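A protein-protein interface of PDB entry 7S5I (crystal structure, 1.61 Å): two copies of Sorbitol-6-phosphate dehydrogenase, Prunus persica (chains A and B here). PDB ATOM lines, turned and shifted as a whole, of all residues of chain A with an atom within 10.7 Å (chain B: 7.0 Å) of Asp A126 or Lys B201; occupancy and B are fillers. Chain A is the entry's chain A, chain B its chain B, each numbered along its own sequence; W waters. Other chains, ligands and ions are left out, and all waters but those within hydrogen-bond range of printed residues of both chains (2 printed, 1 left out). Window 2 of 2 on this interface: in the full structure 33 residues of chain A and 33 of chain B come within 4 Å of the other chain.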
ATOM      1  N   LEU A 111     -22.099 -16.628   7.870  1.00  0.00           N
ATOM      2  CA  LEU A 111     -22.855 -16.387   9.096  1.00  0.00           C
ATOM      3  C   LEU A 111     -23.741 -15.176   8.861  1.00  0.00           C
ATOM      4  O   LEU A 111     -23.234 -14.107   8.509  1.00  0.00           O
ATOM      5  CB  LEU A 111     -21.913 -16.129  10.287  1.00  0.00           C
ATOM      6  CG  LEU A 111     -22.603 -16.019  11.651  1.00  0.00           C
ATOM      7  CD1 LEU A 111     -22.968 -17.384  12.189  1.00  0.00           C
ATOM      8  CD2 LEU A 111     -21.656 -15.300  12.632  1.00  0.00           C
ATOM      9  N   ALA A 112     -25.049 -15.335   9.064  1.00  0.00           N
ATOM     10  CA  ALA A 112     -25.981 -14.213   9.002  1.00  0.00           C
ATOM     11  C   ALA A 112     -26.312 -13.766  10.418  1.00  0.00           C
ATOM     12  O   ALA A 112     -26.563 -14.603  11.280  1.00  0.00           O
ATOM     13  CB  ALA A 112     -27.279 -14.614   8.295  1.00  0.00           C
ATOM     14  N   THR A 113     -26.307 -12.452  10.653  1.00  0.00           N
ATOM     15  CA  THR A 113     -26.728 -11.878  11.926  1.00  0.00           C
ATOM     16  C   THR A 113     -27.756 -10.780  11.665  1.00  0.00           C
ATOM     17  O   THR A 113     -28.027 -10.417  10.519  1.00  0.00           O
ATOM     18  CB  THR A 113     -25.528 -11.341  12.738  1.00  0.00           C
ATOM     19  OG1 THR A 113     -24.902 -10.283  12.017  1.00  0.00           O
ATOM     20  CG2 THR A 113     -24.475 -12.448  13.006  1.00  0.00           C
ATOM     21  N   LYS A 114     -28.337 -10.260  12.747  1.00  0.00           N
ATOM     22  CA  LYS A 114     -29.466  -9.329  12.637  1.00  0.00           C
ATOM     23  C   LYS A 114     -29.098  -8.101  11.806  1.00  0.00           C
ATOM     24  O   LYS A 114     -28.056  -7.477  12.006  1.00  0.00           O
ATOM     25  CB  LYS A 114     -29.938  -8.876  14.012  1.00  0.00           C
ATOM     26  CG  LYS A 114     -31.235  -8.079  13.951  1.00  0.00           C
ATOM     27  CD  LYS A 114     -31.711  -7.685  15.343  1.00  0.00           C
ATOM     28  CE  LYS A 114     -33.044  -6.936  15.285  1.00  0.00           C
ATOM     29  NZ  LYS A 114     -34.148  -7.781  14.754  1.00  0.00           N
ATOM     30  N   ALA A 122     -23.232  -3.860  11.464  1.00  0.00           N
ATOM     31  CA  ALA A 122     -23.028  -4.034  12.895  1.00  0.00           C
ATOM     32  C   ALA A 122     -23.137  -5.505  13.221  1.00  0.00           C
ATOM     33  O   ALA A 122     -23.632  -6.299  12.419  1.00  0.00           O
ATOM     34  CB  ALA A 122     -24.051  -3.232  13.718  1.00  0.00           C
ATOM     35  N   SER A 123     -22.613  -5.866  14.398  1.00  0.00           N
ATOM     36  CA  SER A 123     -22.771  -7.216  14.946  1.00  0.00           C
ATOM     37  C   SER A 123     -23.627  -7.060  16.204  1.00  0.00           C
ATOM     38  O   SER A 123     -23.119  -6.793  17.299  1.00  0.00           O
ATOM     39  CB  SER A 123     -21.426  -7.842  15.233  1.00  0.00           C
ATOM     40  OG  SER A 123     -20.722  -8.057  14.009  1.00  0.00           O
ATOM     41  N   LEU A 124     -24.945  -7.165  16.028  1.00  0.00           N
ATOM     42  CA  LEU A 124     -25.869  -6.848  17.097  1.00  0.00           C
ATOM     43  C   LEU A 124     -25.981  -8.013  18.070  1.00  0.00           C
ATOM     44  O   LEU A 124     -25.877  -9.184  17.674  1.00  0.00           O
ATOM     45  CB  LEU A 124     -27.251  -6.516  16.534  1.00  0.00           C
ATOM     46  CG  LEU A 124     -27.249  -5.295  15.608  1.00  0.00           C
ATOM     47  CD1 LEU A 124     -28.634  -5.144  14.983  1.00  0.00           C
ATOM     48  CD2 LEU A 124     -26.821  -4.011  16.298  1.00  0.00           C
ATOM     49  N   LEU A 125     -26.179  -7.688  19.340  1.00  0.00           N
ATOM     50  CA  LEU A 125     -26.318  -8.704  20.381  1.00  0.00           C
ATOM     51  C   LEU A 125     -27.778  -8.868  20.781  1.00  0.00           C
ATOM     52  O   LEU A 125     -28.572  -7.926  20.699  1.00  0.00           O
ATOM     53  CB  LEU A 125     -25.509  -8.336  21.626  1.00  0.00           C
ATOM     54  CG  LEU A 125     -24.035  -8.026  21.371  1.00  0.00           C
ATOM     55  CD1 LEU A 125     -23.357  -7.733  22.703  1.00  0.00           C
ATOM     56  CD2 LEU A 125     -23.338  -9.165  20.636  1.00  0.00           C
ATOM     57  N   ASP A 126     -28.118 -10.060  21.271  1.00  0.00           N
ATOM     58  CA  ASP A 126     -29.470 -10.313  21.745  1.00  0.00           C
ATOM     59  C   ASP A 126     -29.595  -9.883  23.205  1.00  0.00           C
ATOM     60  O   ASP A 126     -28.697  -9.250  23.777  1.00  0.00           O
ATOM     61  CB  ASP A 126     -29.843 -11.779  21.526  1.00  0.00           C
ATOM     62  CG  ASP A 126     -29.098 -12.737  22.455  1.00  0.00           C
ATOM     63  OD1 ASP A 126     -28.409 -12.306  23.407  1.00  0.00           O
ATOM     64  OD2 ASP A 126     -29.205 -13.957  22.214  1.00  0.00           O
ATOM     65  N   GLU A 127     -30.720 -10.270  23.822  1.00  0.00           N
ATOM     66  CA  GLU A 127     -31.044  -9.876  25.193  1.00  0.00           C
ATOM     67  C   GLU A 127     -30.016 -10.385  26.195  1.00  0.00           C
ATOM     68  O   GLU A 127     -29.850  -9.798  27.274  1.00  0.00           O
ATOM     69  CB  GLU A 127     -32.429 -10.410  25.550  1.00  0.00           C
ATOM     70  CG  GLU A 127     -32.606 -11.875  25.141  1.00  0.00           C
ATOM     71  CD  GLU A 127     -33.929 -12.475  25.575  1.00  0.00           C
ATOM     72  OE1 GLU A 127     -34.325 -13.509  24.993  1.00  0.00           O
ATOM     73  OE2 GLU A 127     -34.563 -11.933  26.507  1.00  0.00           O
ATOM     74  N   ASN A 128     -29.344 -11.489  25.877  1.00  0.00           N
ATOM     75  CA  ASN A 128     -28.340 -12.084  26.744  1.00  0.00           C
ATOM     76  C   ASN A 128     -26.913 -11.696  26.363  1.00  0.00           C
ATOM     77  O   ASN A 128     -25.967 -12.325  26.843  1.00  0.00           O
ATOM     78  CB  ASN A 128     -28.495 -13.605  26.744  1.00  0.00           C
ATOM     79  CG  ASN A 128     -29.942 -14.044  26.916  1.00  0.00           C
ATOM     80  OD1 ASN A 128     -30.426 -14.927  26.210  1.00  0.00           O
ATOM     81  ND2 ASN A 128     -30.633 -13.431  27.868  1.00  0.00           N
ATOM     82  N   LYS A 129     -26.738 -10.664  25.528  1.00  0.00           N
ATOM     83  CA  LYS A 129     -25.416 -10.182  25.112  1.00  0.00           C
ATOM     84  C   LYS A 129     -24.666 -11.237  24.309  1.00  0.00           C
ATOM     85  O   LYS A 129     -23.430 -11.306  24.333  1.00  0.00           O
ATOM     86  CB  LYS A 129     -24.573  -9.714  26.301  1.00  0.00           C
ATOM     87  CG  LYS A 129     -25.230  -8.631  27.133  1.00  0.00           C
ATOM     88  CD  LYS A 129     -25.440  -7.357  26.333  1.00  0.00           C
ATOM     89  CE  LYS A 129     -26.209  -6.315  27.146  1.00  0.00           C
ATOM     90  NZ  LYS A 129     -27.687  -6.509  27.079  1.00  0.00           N
ATOM     91  N   VAL A 130     -25.421 -12.043  23.579  1.00  0.00           N
ATOM     92  CA  VAL A 130     -24.886 -13.042  22.662  1.00  0.00           C
ATOM     93  C   VAL A 130     -25.222 -12.595  21.250  1.00  0.00           C
ATOM     94  O   VAL A 130     -26.321 -12.090  21.001  1.00  0.00           O
ATOM     95  CB  VAL A 130     -25.484 -14.425  22.982  1.00  0.00           C
ATOM     96  CG1 VAL A 130     -25.156 -15.419  21.901  1.00  0.00           C
ATOM     97  CG2 VAL A 130     -24.960 -14.912  24.333  1.00  0.00           C
ATOM     98  N   LEU A 131     -24.269 -12.754  20.325  1.00  0.00           N
ATOM     99  CA  LEU A 131     -24.489 -12.356  18.937  1.00  0.00           C
ATOM    100  C   LEU A 131     -25.858 -12.804  18.445  1.00  0.00           C
ATOM    101  O   LEU A 131     -26.250 -13.961  18.622  1.00  0.00           O
ATOM    102  CB  LEU A 131     -23.399 -12.964  18.054  1.00  0.00           C
ATOM    103  CG  LEU A 131     -23.327 -12.497  16.609  1.00  0.00           C
ATOM    104  CD1 LEU A 131     -22.978 -11.011  16.505  1.00  0.00           C
ATOM    105  CD2 LEU A 131     -22.281 -13.356  15.849  1.00  0.00           C
ATOM    106  N   ASP A 132     -26.600 -11.866  17.848  1.00  0.00           N
ATOM    107  CA  ASP A 132     -27.965 -12.145  17.409  1.00  0.00           C
ATOM    108  C   ASP A 132     -27.889 -12.824  16.044  1.00  0.00           C
ATOM    109  O   ASP A 132     -28.072 -12.217  14.986  1.00  0.00           O
ATOM    110  CB  ASP A 132     -28.787 -10.860  17.380  1.00  0.00           C
ATOM    111  CG  ASP A 132     -30.274 -11.125  17.280  1.00  0.00           C
ATOM    112  OD1 ASP A 132     -30.657 -12.293  17.088  1.00  0.00           O
ATOM    113  OD2 ASP A 132     -31.061 -10.163  17.390  1.00  0.00           O
ATOM    114  N   ILE A 133     -27.571 -14.117  16.081  1.00  0.00           N
ATOM    115  CA  ILE A 133     -27.398 -14.908  14.866  1.00  0.00           C
ATOM    116  C   ILE A 133     -28.756 -15.203  14.234  1.00  0.00           C
ATOM    117  O   ILE A 133     -29.688 -15.666  14.903  1.00  0.00           O
ATOM    118  CB  ILE A 133     -26.624 -16.198  15.200  1.00  0.00           C
ATOM    119  CG1 ILE A 133     -25.186 -15.842  15.617  1.00  0.00           C
ATOM    120  CG2 ILE A 133     -26.603 -17.152  14.006  1.00  0.00           C
ATOM    121  CD1 ILE A 133     -24.409 -17.038  16.218  1.00  0.00           C
ATOM    122  N   ASP A 134     -28.872 -14.907  12.933  1.00  0.00           N
ATOM    123  CA  ASP A 134     -30.111 -15.067  12.190  1.00  0.00           C
ATOM    124  C   ASP A 134     -30.322 -16.520  11.779  1.00  0.00           C
ATOM    125  O   ASP A 134     -29.368 -17.229  11.446  1.00  0.00           O
ATOM    126  CB  ASP A 134     -30.047 -14.170  10.949  1.00  0.00           C
ATOM    127  CG  ASP A 134     -31.098 -14.535   9.940  1.00  0.00           C
ATOM    128  OD1 ASP A 134     -30.836 -15.429   9.106  1.00  0.00           O
ATOM    129  OD2 ASP A 134     -32.189 -13.933  10.004  1.00  0.00           O
ATOM    130  N   VAL A 135     -31.583 -16.971  11.799  1.00  0.00           N
ATOM    131  CA  VAL A 135     -31.889 -18.328  11.345  1.00  0.00           C
ATOM    132  C   VAL A 135     -33.017 -18.283  10.321  1.00  0.00           C
ATOM    133  O   VAL A 135     -33.886 -19.172  10.284  1.00  0.00           O
ATOM    134  CB  VAL A 135     -32.227 -19.273  12.516  1.00  0.00           C
ATOM    135  CG1 VAL A 135     -30.972 -19.490  13.374  1.00  0.00           C
ATOM    136  CG2 VAL A 135     -33.369 -18.732  13.388  1.00  0.00           C
ATOM    137  N   SER A 303     -16.358  -9.889  21.976  1.00  0.00           N
ATOM    138  CA  SER A 303     -17.624  -9.216  22.242  1.00  0.00           C
ATOM    139  C   SER A 303     -18.802  -9.861  21.520  1.00  0.00           C
ATOM    140  O   SER A 303     -19.943  -9.562  21.877  1.00  0.00           O
ATOM    141  CB  SER A 303     -17.546  -7.734  21.867  1.00  0.00           C
ATOM    142  OG  SER A 303     -17.565  -7.564  20.463  1.00  0.00           O
ATOM    143  N   TRP A 304     -18.577 -10.744  20.543  1.00  0.00           N
ATOM    144  CA  TRP A 304     -19.706 -11.488  19.980  1.00  0.00           C
ATOM    145  C   TRP A 304     -20.362 -12.379  21.018  1.00  0.00           C
ATOM    146  O   TRP A 304     -21.538 -12.729  20.875  1.00  0.00           O
ATOM    147  CB  TRP A 304     -19.268 -12.367  18.808  1.00  0.00           C
ATOM    148  CG  TRP A 304     -18.949 -11.641  17.545  1.00  0.00           C
ATOM    149  CD1 TRP A 304     -18.826 -10.305  17.378  1.00  0.00           C
ATOM    150  CD2 TRP A 304     -18.686 -12.236  16.265  1.00  0.00           C
ATOM    151  NE1 TRP A 304     -18.504 -10.014  16.060  1.00  0.00           N
ATOM    152  CE2 TRP A 304     -18.424 -11.187  15.359  1.00  0.00           C
ATOM    153  CE3 TRP A 304     -18.687 -13.556  15.793  1.00  0.00           C
ATOM    154  CZ2 TRP A 304     -18.133 -11.420  14.009  1.00  0.00           C
ATOM    155  CZ3 TRP A 304     -18.399 -13.787  14.430  1.00  0.00           C
ATOM    156  CH2 TRP A 304     -18.127 -12.725  13.573  1.00  0.00           C
ATOM    157  N   GLY A 305     -19.618 -12.807  22.035  1.00  0.00           N
ATOM    158  CA  GLY A 305     -20.198 -13.726  23.011  1.00  0.00           C
ATOM    159  C   GLY A 305     -20.470 -15.123  22.492  1.00  0.00           C
ATOM    160  O   GLY A 305     -21.221 -15.883  23.124  1.00  0.00           O
ATOM    161  N   VAL A 306     -19.901 -15.463  21.338  1.00  0.00           N
ATOM    162  CA  VAL A 306     -20.083 -16.737  20.660  1.00  0.00           C
ATOM    163  C   VAL A 306     -18.755 -17.069  20.012  1.00  0.00           C
ATOM    164  O   VAL A 306     -18.167 -16.214  19.340  1.00  0.00           O
ATOM    165  CB  VAL A 306     -21.166 -16.679  19.566  1.00  0.00           C
ATOM    166  CG1 VAL A 306     -21.251 -18.035  18.850  1.00  0.00           C
ATOM    167  CG2 VAL A 306     -22.498 -16.313  20.129  1.00  0.00           C
ATOM    168  N   LYS B 178     -37.489 -28.468  11.436  1.00  0.00           N
ATOM    169  CA  LYS B 178     -36.302 -28.142  12.217  1.00  0.00           C
ATOM    170  C   LYS B 178     -35.692 -29.427  12.766  1.00  0.00           C
ATOM    171  O   LYS B 178     -36.424 -30.293  13.252  1.00  0.00           O
ATOM    172  CB  LYS B 178     -36.682 -27.202  13.360  1.00  0.00           C
ATOM    173  CG  LYS B 178     -35.605 -26.918  14.397  1.00  0.00           C
ATOM    174  CD  LYS B 178     -35.929 -25.638  15.161  1.00  0.00           C
ATOM    175  CE  LYS B 178     -37.021 -25.849  16.201  1.00  0.00           C
ATOM    176  NZ  LYS B 178     -37.190 -24.617  17.020  1.00  0.00           N
ATOM    177  N   LEU B 195     -21.527 -23.969  20.831  1.00  0.00           N
ATOM    178  CA  LEU B 195     -22.320 -24.755  19.905  1.00  0.00           C
ATOM    179  C   LEU B 195     -23.469 -25.424  20.632  1.00  0.00           C
ATOM    180  O   LEU B 195     -24.601 -25.450  20.133  1.00  0.00           O
ATOM    181  CB  LEU B 195     -21.432 -25.786  19.215  1.00  0.00           C
ATOM    182  CG  LEU B 195     -22.137 -26.711  18.231  1.00  0.00           C
ATOM    183  CD1 LEU B 195     -22.800 -25.870  17.123  1.00  0.00           C
ATOM    184  CD2 LEU B 195     -21.146 -27.695  17.629  1.00  0.00           C
ATOM    185  N   VAL B 196     -23.183 -25.957  21.818  1.00  0.00           N
ATOM    186  CA  VAL B 196     -24.223 -26.519  22.671  1.00  0.00           C
ATOM    187  C   VAL B 196     -25.283 -25.470  22.974  1.00  0.00           C
ATOM    188  O   VAL B 196     -26.487 -25.729  22.865  1.00  0.00           O
ATOM    189  CB  VAL B 196     -23.585 -27.088  23.950  1.00  0.00           C
ATOM    190  CG1 VAL B 196     -24.656 -27.478  24.978  1.00  0.00           C
ATOM    191  CG2 VAL B 196     -22.743 -28.295  23.574  1.00  0.00           C
ATOM    192  N   ARG B 197     -24.849 -24.262  23.345  1.00  0.00           N
ATOM    193  CA  ARG B 197     -25.799 -23.210  23.694  1.00  0.00           C
ATOM    194  C   ARG B 197     -26.613 -22.781  22.477  1.00  0.00           C
ATOM    195  O   ARG B 197     -27.818 -22.514  22.590  1.00  0.00           O
ATOM    196  CB  ARG B 197     -25.044 -22.027  24.300  1.00  0.00           C
ATOM    197  CG  ARG B 197     -24.754 -22.214  25.796  1.00  0.00           C
ATOM    198  CD  ARG B 197     -24.289 -20.909  26.436  1.00  0.00           C
ATOM    199  NE  ARG B 197     -23.972 -21.023  27.856  1.00  0.00           N
ATOM    200  CZ  ARG B 197     -24.791 -20.658  28.835  1.00  0.00           C
ATOM    201  NH1 ARG B 197     -26.000 -20.178  28.586  1.00  0.00           N
ATOM    202  NH2 ARG B 197     -24.386 -20.773  30.097  1.00  0.00           N
ATOM    203  N   PHE B 198     -25.981 -22.733  21.303  1.00  0.00           N
ATOM    204  CA  PHE B 198     -26.697 -22.321  20.100  1.00  0.00           C
ATOM    205  C   PHE B 198     -27.786 -23.321  19.737  1.00  0.00           C
ATOM    206  O   PHE B 198     -28.915 -22.931  19.432  1.00  0.00           O
ATOM    207  CB  PHE B 198     -25.717 -22.144  18.930  1.00  0.00           C
ATOM    208  CG  PHE B 198     -26.377 -21.733  17.644  1.00  0.00           C
ATOM    209  CD1 PHE B 198     -26.745 -20.412  17.416  1.00  0.00           C
ATOM    210  CD2 PHE B 198     -26.648 -22.685  16.664  1.00  0.00           C
ATOM    211  CE1 PHE B 198     -27.366 -20.036  16.216  1.00  0.00           C
ATOM    212  CE2 PHE B 198     -27.266 -22.331  15.481  1.00  0.00           C
ATOM    213  CZ  PHE B 198     -27.636 -21.009  15.254  1.00  0.00           C
ATOM    214  N   CYS B 199     -27.456 -24.614  19.757  1.00  0.00           N
ATOM    215  CA  CYS B 199     -28.453 -25.650  19.506  1.00  0.00           C
ATOM    216  C   CYS B 199     -29.636 -25.500  20.450  1.00  0.00           C
ATOM    217  O   CYS B 199     -30.788 -25.462  20.006  1.00  0.00           O
ATOM    218  CB  CYS B 199     -27.822 -27.038  19.669  1.00  0.00           C
ATOM    219  SG  CYS B 199     -26.731 -27.519  18.334  1.00  0.00           S
ATOM    220  N   LYS B 200     -29.358 -25.373  21.754  1.00  0.00           N
ATOM    221  CA  LYS B 200     -30.417 -25.295  22.758  1.00  0.00           C
ATOM    222  C   LYS B 200     -31.274 -24.052  22.564  1.00  0.00           C
ATOM    223  O   LYS B 200     -32.501 -24.109  22.730  1.00  0.00           O
ATOM    224  CB  LYS B 200     -29.816 -25.337  24.164  1.00  0.00           C
ATOM    225  CG  LYS B 200     -29.203 -26.700  24.492  1.00  0.00           C
ATOM    226  CD  LYS B 200     -28.320 -26.666  25.735  1.00  0.00           C
ATOM    227  CE  LYS B 200     -29.135 -26.664  27.007  1.00  0.00           C
ATOM    228  NZ  LYS B 200     -28.240 -26.564  28.202  1.00  0.00           N
ATOM    229  N   LYS B 201     -30.644 -22.918  22.223  1.00  0.00           N
ATOM    230  CA  LYS B 201     -31.396 -21.691  21.976  1.00  0.00           C
ATOM    231  C   LYS B 201     -32.479 -21.915  20.929  1.00  0.00           C
ATOM    232  O   LYS B 201     -33.577 -21.348  21.022  1.00  0.00           O
ATOM    233  CB  LYS B 201     -30.449 -20.576  21.525  1.00  0.00           C
ATOM    234  CG  LYS B 201     -31.190 -19.311  21.095  1.00  0.00           C
ATOM    235  CD  LYS B 201     -30.244 -18.161  20.814  1.00  0.00           C
ATOM    236  CE  LYS B 201     -31.006 -16.916  20.429  1.00  0.00           C
ATOM    237  NZ  LYS B 201     -30.069 -15.838  19.971  1.00  0.00           N
ATOM    238  N   HIS B 202     -32.187 -22.727  19.919  1.00  0.00           N
ATOM    239  CA  HIS B 202     -33.108 -22.940  18.814  1.00  0.00           C
ATOM    240  C   HIS B 202     -33.862 -24.255  18.914  1.00  0.00           C
ATOM    241  O   HIS B 202     -34.413 -24.712  17.909  1.00  0.00           O
ATOM    242  CB  HIS B 202     -32.350 -22.832  17.496  1.00  0.00           C
ATOM    243  CG  HIS B 202     -31.859 -21.455  17.252  1.00  0.00           C
ATOM    244  ND1 HIS B 202     -32.696 -20.435  16.854  1.00  0.00           N
ATOM    245  CD2 HIS B 202     -30.645 -20.893  17.456  1.00  0.00           C
ATOM    246  CE1 HIS B 202     -32.003 -19.313  16.776  1.00  0.00           C
ATOM    247  NE2 HIS B 202     -30.757 -19.567  17.133  1.00  0.00           N
ATOM    248  N   GLY B 203     -33.895 -24.868  20.098  1.00  0.00           N
ATOM    249  CA  GLY B 203     -34.744 -26.031  20.298  1.00  0.00           C
ATOM    250  C   GLY B 203     -34.220 -27.321  19.717  1.00  0.00           C
ATOM    251  O   GLY B 203     -34.988 -28.268  19.528  1.00  0.00           O
ATOM    252  N   VAL B 204     -32.929 -27.382  19.421  1.00  0.00           N
ATOM    253  CA  VAL B 204     -32.263 -28.584  18.938  1.00  0.00           C
ATOM    254  C   VAL B 204     -31.545 -29.203  20.127  1.00  0.00           C
ATOM    255  O   VAL B 204     -30.838 -28.493  20.855  1.00  0.00           O
ATOM    256  CB  VAL B 204     -31.269 -28.238  17.810  1.00  0.00           C
ATOM    257  CG1 VAL B 204     -30.608 -29.500  17.262  1.00  0.00           C
ATOM    258  CG2 VAL B 204     -31.960 -27.463  16.688  1.00  0.00           C
HETATM  259  O   HOH W   1     -27.090 -16.882  19.011  1.00  0.00           O
HETATM  260  O   HOH W   2     -29.424 -17.055  17.306  1.00  0.00           O
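CG2 of Ile A133 touches CE1 of Phe B198 (3.7 Å). His B202 touches Val A135 (CE1 to CG1, 3.6 Å).
The side-chain amino group (NZ) of Lys B201 is in salt-bridge range of the side-chain carboxylate (OD2) of Asp A126.
Hydrophobic or aromatic side chains of chain A that line the printed part of chain B: Ile A133 and Val A135. Of the 11 printed residues of chain B, 3 touch a printed residue of chain A. Hydrophobic or aromatic side chains of chain B within 4 Å of the printed part of chain A: Phe B198 and His B202. Along chain B the printed residues that touch a printed residue of chain A span positions 198 to 202. Among the printed residues, Asp or Glu carboxylates within 4 Å of a Lys or Arg side-chain nitrogen of the other chain: Asp A126 with Lys B201 (3.1 Å).
Water W2 lies within hydrogen-bond range of O of Ile A133 (2.8 Å), NE2 of His B202 (2.8 Å) and NZ of Lys B201 (3.0 Å). Water W1 bridges the backbone carbonyl oxygen of Leu A131 (3.1 Å) and the side-chain amino group of Lys B201 (3.3 Å).
Of the printed residues of chain B, Asp A126 touches Lys B201. Lys B201 touches just one residue of chain A: Asp A126 (3.1 Å). Of chain A, only Val A135 (3.6 Å) comes within 4 Å of His B202. Of the printed residues of chain B, Ile A133 touches Phe B198 (3.7 Å). Of the printed residues of chain A, Phe B198 touches Ile A133. Of the printed residues of chain B, Val A135 touches His B202. Leu A131 touches none of the printed residues of chain B. The nearest printed residue of chain B that does not touch Asp A126 is His B202 (7.7 Å). The nearest residue of chain A that does not touch Lys B201 is Leu A131 (4.5 Å).
No position is printed for both chains. Of the 3 pairs that touch across the chains among the printed residues, none has its exchanged pair printed and touching as well.
OD1 of Asp A126 is in hydrogen-bond range of N of Lys A129, 3.2 Å away. The backbone NH (N) of Val A130 sits at hydrogen-bond distance from the side-chain carboxylate (OD1) of Asp A126. The side-chain amino group (NZ) of Lys B178 sits at hydrogen-bond distance from the backbone carbonyl oxygen (O) of His B202 (2.9 Å). The side-chain carboxylate (OD1) of Asp A126 lies within hydrogen-bond range of the backbone NH (N) of Asn A128.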
